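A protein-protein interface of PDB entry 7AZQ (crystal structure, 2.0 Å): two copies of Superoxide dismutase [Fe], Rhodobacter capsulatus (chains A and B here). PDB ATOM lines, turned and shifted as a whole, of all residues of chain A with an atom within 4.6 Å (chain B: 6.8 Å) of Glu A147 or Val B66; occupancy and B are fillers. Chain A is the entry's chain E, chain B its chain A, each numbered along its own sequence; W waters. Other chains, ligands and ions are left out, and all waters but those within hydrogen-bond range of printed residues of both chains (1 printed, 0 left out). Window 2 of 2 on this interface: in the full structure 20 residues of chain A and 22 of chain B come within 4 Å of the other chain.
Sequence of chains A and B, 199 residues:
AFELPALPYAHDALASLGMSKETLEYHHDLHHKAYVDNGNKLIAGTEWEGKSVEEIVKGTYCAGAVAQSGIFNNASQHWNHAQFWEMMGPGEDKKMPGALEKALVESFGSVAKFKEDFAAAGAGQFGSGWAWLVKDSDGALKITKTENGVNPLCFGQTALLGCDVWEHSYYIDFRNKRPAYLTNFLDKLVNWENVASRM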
ATOM      1  N   ALA A  65     -28.782  -8.747  11.118  1.00  0.00           N
ATOM      2  CA  ALA A  65     -27.350  -8.560  11.351  1.00  0.00           C
ATOM      3  C   ALA A  65     -26.724  -9.749  12.092  1.00  0.00           C
ATOM      4  O   ALA A  65     -27.309 -10.287  13.016  1.00  0.00           O
ATOM      5  CB  ALA A  65     -27.125  -7.272  12.117  1.00  0.00           C
ATOM      6  N   VAL A  66     -25.496 -10.089  11.701  1.00  0.00           N
ATOM      7  CA  VAL A  66     -24.701 -11.135  12.348  1.00  0.00           C
ATOM      8  C   VAL A  66     -24.282 -10.700  13.739  1.00  0.00           C
ATOM      9  O   VAL A  66     -24.344 -11.483  14.667  1.00  0.00           O
ATOM     10  CB  VAL A  66     -23.478 -11.424  11.455  1.00  0.00           C
ATOM     11  CG1 VAL A  66     -22.445 -12.296  12.154  1.00  0.00           C
ATOM     12  CG2 VAL A  66     -23.975 -12.075  10.161  1.00  0.00           C
ATOM     13  N   GLN A 125     -25.495 -24.905  20.735  1.00  0.00           N
ATOM     14  CA  GLN A 125     -25.231 -23.506  20.404  1.00  0.00           C
ATOM     15  C   GLN A 125     -23.725 -23.339  20.287  1.00  0.00           C
ATOM     16  O   GLN A 125     -23.031 -23.317  21.291  1.00  0.00           O
ATOM     17  CB  GLN A 125     -25.798 -22.564  21.454  1.00  0.00           C
ATOM     18  CG  GLN A 125     -25.621 -21.095  21.117  1.00  0.00           C
ATOM     19  CD  GLN A 125     -26.316 -20.704  19.849  1.00  0.00           C
ATOM     20  OE1 GLN A 125     -27.430 -21.190  19.575  1.00  0.00           O
ATOM     21  NE2 GLN A 125     -25.690 -19.822  19.072  1.00  0.00           N
ATOM     22  N   SER A 128     -20.932 -18.737  22.065  1.00  0.00           N
ATOM     23  CA  SER A 128     -21.542 -18.216  23.284  1.00  0.00           C
ATOM     24  C   SER A 128     -23.037 -18.072  23.030  1.00  0.00           C
ATOM     25  O   SER A 128     -23.462 -17.755  21.890  1.00  0.00           O
ATOM     26  CB  SER A 128     -20.972 -16.851  23.648  1.00  0.00           C
ATOM     27  OG  SER A 128     -19.580 -16.874  23.849  1.00  0.00           O
ATOM     28  N   GLY A 129     -23.831 -18.244  24.097  1.00  0.00           N
ATOM     29  CA  GLY A 129     -25.268 -18.064  24.017  1.00  0.00           C
ATOM     30  C   GLY A 129     -26.045 -18.697  25.143  1.00  0.00           C
ATOM     31  O   GLY A 129     -25.529 -18.850  26.263  1.00  0.00           O
ATOM     32  N   THR A 146     -30.079 -19.470  21.401  1.00  0.00           N
ATOM     33  CA  THR A 146     -29.721 -18.192  20.840  1.00  0.00           C
ATOM     34  C   THR A 146     -28.245 -17.890  21.043  1.00  0.00           C
ATOM     35  O   THR A 146     -27.619 -18.435  21.967  1.00  0.00           O
ATOM     36  CB  THR A 146     -30.523 -17.058  21.532  1.00  0.00           C
ATOM     37  OG1 THR A 146     -30.276 -17.063  22.955  1.00  0.00           O
ATOM     38  CG2 THR A 146     -32.024 -17.207  21.240  1.00  0.00           C
ATOM     39  N   GLU A 147     -27.718 -17.022  20.174  1.00  0.00           N
ATOM     40  CA  GLU A 147     -26.360 -16.536  20.259  1.00  0.00           C
ATOM     41  C   GLU A 147     -26.191 -15.338  21.185  1.00  0.00           C
ATOM     42  O   GLU A 147     -27.023 -14.432  21.224  1.00  0.00           O
ATOM     43  CB  GLU A 147     -25.837 -16.172  18.862  1.00  0.00           C
ATOM     44  CG  GLU A 147     -26.329 -14.869  18.208  1.00  0.00           C
ATOM     45  CD  GLU A 147     -27.708 -14.916  17.541  1.00  0.00           C
ATOM     46  OE1 GLU A 147     -28.479 -15.887  17.750  1.00  0.00           O
ATOM     47  OE2 GLU A 147     -28.049 -13.914  16.874  1.00  0.00           O
ATOM     48  N   ASN A 148     -25.049 -15.319  21.879  1.00  0.00           N
ATOM     49  CA  ASN A 148     -24.554 -14.190  22.594  1.00  0.00           C
ATOM     50  C   ASN A 148     -25.614 -13.692  23.616  1.00  0.00           C
ATOM     51  O   ASN A 148     -25.901 -14.410  24.559  1.00  0.00           O
ATOM     52  CB  ASN A 148     -24.058 -13.122  21.621  1.00  0.00           C
ATOM     53  CG  ASN A 148     -23.113 -13.693  20.565  1.00  0.00           C
ATOM     54  OD1 ASN A 148     -23.209 -13.339  19.338  1.00  0.00           O
ATOM     55  ND2 ASN A 148     -22.238 -14.570  20.983  1.00  0.00           N
ATOM     56  N   GLY A 149     -26.146 -12.483  23.434  1.00  0.00           N
ATOM     57  CA  GLY A 149     -27.246 -12.002  24.256  1.00  0.00           C
ATOM     58  C   GLY A 149     -28.673 -12.128  23.735  1.00  0.00           C
ATOM     59  O   GLY A 149     -29.640 -11.807  24.474  1.00  0.00           O
ATOM     60  N   VAL A 150     -28.821 -12.599  22.484  1.00  0.00           N
ATOM     61  CA  VAL A 150     -30.151 -12.731  21.847  1.00  0.00           C
ATOM     62  C   VAL A 150     -30.975 -13.641  22.751  1.00  0.00           C
ATOM     63  O   VAL A 150     -30.425 -14.533  23.420  1.00  0.00           O
ATOM     64  CB  VAL A 150     -30.044 -13.236  20.411  1.00  0.00           C
ATOM     65  CG1 VAL A 150     -31.405 -13.508  19.782  1.00  0.00           C
ATOM     66  CG2 VAL A 150     -29.242 -12.207  19.591  1.00  0.00           C
ATOM     67  N   CYS B  62     -21.300 -19.748   4.920  1.00  0.00           N
ATOM     68  CA  CYS B  62     -22.559 -19.200   4.447  1.00  0.00           C
ATOM     69  C   CYS B  62     -22.544 -17.704   4.813  1.00  0.00           C
ATOM     70  O   CYS B  62     -22.803 -17.325   5.956  1.00  0.00           O
ATOM     71  CB  CYS B  62     -23.738 -19.914   5.086  1.00  0.00           C
ATOM     72  SG  CYS B  62     -25.325 -19.274   4.500  1.00  0.00           S
ATOM     73  N   GLY B  64     -23.312 -14.292   5.692  1.00  0.00           N
ATOM     74  CA  GLY B  64     -24.472 -13.625   6.251  1.00  0.00           C
ATOM     75  C   GLY B  64     -25.292 -14.449   7.229  1.00  0.00           C
ATOM     76  O   GLY B  64     -26.196 -13.907   7.840  1.00  0.00           O
ATOM     77  N   ALA B  65     -24.998 -15.750   7.352  1.00  0.00           N
ATOM     78  CA  ALA B  65     -25.700 -16.584   8.332  1.00  0.00           C
ATOM     79  C   ALA B  65     -25.136 -16.265   9.675  1.00  0.00           C
ATOM     80  O   ALA B  65     -23.928 -16.032   9.815  1.00  0.00           O
ATOM     81  CB  ALA B  65     -25.528 -18.073   8.068  1.00  0.00           C
ATOM     82  N   VAL B  66     -26.013 -16.237  10.687  1.00  0.00           N
ATOM     83  CA  VAL B  66     -25.593 -16.027  12.049  1.00  0.00           C
ATOM     84  C   VAL B  66     -24.919 -17.286  12.566  1.00  0.00           C
ATOM     85  O   VAL B  66     -23.864 -17.233  13.194  1.00  0.00           O
ATOM     86  CB  VAL B  66     -26.798 -15.654  12.935  1.00  0.00           C
ATOM     87  CG1 VAL B  66     -26.366 -15.488  14.368  1.00  0.00           C
ATOM     88  CG2 VAL B  66     -27.413 -14.375  12.402  1.00  0.00           C
ATOM     89  N   ALA B  67     -25.575 -18.424  12.328  1.00  0.00           N
ATOM     90  CA  ALA B  67     -25.071 -19.733  12.690  1.00  0.00           C
ATOM     91  C   ALA B  67     -24.626 -20.452  11.406  1.00  0.00           C
ATOM     92  O   ALA B  67     -25.356 -20.453  10.430  1.00  0.00           O
ATOM     93  CB  ALA B  67     -26.159 -20.520  13.413  1.00  0.00           C
ATOM     94  N   GLN B  68     -23.403 -20.992  11.418  1.00  0.00           N
ATOM     95  CA  GLN B  68     -22.843 -21.706  10.283  1.00  0.00           C
ATOM     96  C   GLN B  68     -23.141 -23.209  10.512  1.00  0.00           C
ATOM     97  O   GLN B  68     -23.614 -23.588  11.578  1.00  0.00           O
ATOM     98  CB  GLN B  68     -21.328 -21.472  10.223  1.00  0.00           C
ATOM     99  CG  GLN B  68     -20.906 -20.021  10.072  1.00  0.00           C
ATOM    100  CD  GLN B  68     -21.302 -19.419   8.738  1.00  0.00           C
ATOM    101  OE1 GLN B  68     -21.353 -20.125   7.701  1.00  0.00           O
ATOM    102  NE2 GLN B  68     -21.552 -18.103   8.728  1.00  0.00           N
ATOM    103  N   GLU B 147     -16.592 -13.846  14.476  1.00  0.00           N
ATOM    104  CA  GLU B 147     -17.357 -14.684  15.409  1.00  0.00           C
ATOM    105  C   GLU B 147     -17.026 -16.157  15.301  1.00  0.00           C
ATOM    106  O   GLU B 147     -16.814 -16.697  14.210  1.00  0.00           O
ATOM    107  CB  GLU B 147     -18.870 -14.489  15.233  1.00  0.00           C
ATOM    108  CG  GLU B 147     -19.483 -15.059  13.945  1.00  0.00           C
ATOM    109  CD  GLU B 147     -19.319 -14.193  12.700  1.00  0.00           C
ATOM    110  OE1 GLU B 147     -18.687 -13.080  12.781  1.00  0.00           O
ATOM    111  OE2 GLU B 147     -19.810 -14.612  11.617  1.00  0.00           O
ATOM    112  N   ASN B 148     -17.022 -16.816  16.452  1.00  0.00           N
ATOM    113  CA  ASN B 148     -16.989 -18.266  16.565  1.00  0.00           C
ATOM    114  C   ASN B 148     -15.771 -18.844  15.824  1.00  0.00           C
ATOM    115  O   ASN B 148     -14.632 -18.592  16.233  1.00  0.00           O
ATOM    116  CB  ASN B 148     -18.355 -18.820  16.114  1.00  0.00           C
ATOM    117  CG  ASN B 148     -19.532 -18.131  16.836  1.00  0.00           C
ATOM    118  OD1 ASN B 148     -19.457 -17.893  18.052  1.00  0.00           O
ATOM    119  ND2 ASN B 148     -20.598 -17.839  16.118  1.00  0.00           N
ATOM    120  N   VAL B 150     -15.414 -18.335  12.296  1.00  0.00           N
ATOM    121  CA  VAL B 150     -15.232 -17.531  11.094  1.00  0.00           C
ATOM    122  C   VAL B 150     -13.822 -16.955  11.150  1.00  0.00           C
ATOM    123  O   VAL B 150     -13.295 -16.688  12.222  1.00  0.00           O
ATOM    124  CB  VAL B 150     -16.357 -16.466  10.941  1.00  0.00           C
ATOM    125  CG1 VAL B 150     -16.129 -15.528   9.755  1.00  0.00           C
ATOM    126  CG2 VAL B 150     -17.711 -17.158  10.798  1.00  0.00           C
HETATM  127  O   HOH W   1     -20.368 -16.539  20.238  1.00  0.00           O
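Printed residues of chain A that touch a printed residue of chain B: Val A66 and Glu A147.
Hydrophobic or aromatic side chains of chain B within 4 Å of the printed part of chain A: Val B66.
Along chain B the printed residues that touch a printed residue of chain A span positions 64 to 147.
Among the printed residues, 4 pairs touch across the chains.
Among the printed residues, no Asp or Glu carboxylate lies within 4 Å of a Lys or Arg side-chain nitrogen of the other chain.
The backbone carbonyl oxygen (O) of Ala B65 lies within hydrogen-bond range of the side-chain amide nitrogen (NE2) of Gln B68, at 3.3 Å.
Of the printed residues of chain B, Val A66 touches Gly B64 (3.7 Å), Ala B65 (3.97 Å) and Glu B147 (3.5 Å).
Glu A147 touches just one residue of chain B: Val B66 (3.4 Å).
Gly A149 touches none of the printed residues of chain B.
Of the printed residues of chain A, Gly B64 touches Val A66.
Printed residues of chain A within 4 Å of Ala B65: Val A66 (3.97 Å).
Of chain A, only Glu A147 (3.4 Å) comes within 4 Å of Val B66.
Gln B68 touches none of the printed residues of chain A.
Of the printed residues of chain A, Glu B147 touches Val A66 (3.5 Å).
The nearest residue of chain B that does not touch Glu A147 is Asn B148 (6.1 Å).
The nearest residue of chain A that does not touch Val B66 is Ala A65 (4.1 Å).
The nearest printed residue of chain B that does not touch Val A66 is Val B66 (4.2 Å).
Val A66 touches Ala B65, but with the chains exchanged Ala A65 does not touch Val B66 (4.1 Å).
Val A66 touches Glu B147, and with the chains exchanged Glu A147 touches Val B66.
Val A66 touches Gly B64 (CG2 to O, 3.7 Å).
Val A66 touches Ala B65.
Val A66 touches Glu B147.
CG1 of Val B66 touches OE2 of Glu A147, at 3.4 Å.
Water W1 lies within hydrogen-bond range of OD1 of Asn B148 (2.7 Å), ND2 of Asn A148 (2.8 Å) and N of Ser A128 (2.9 Å).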
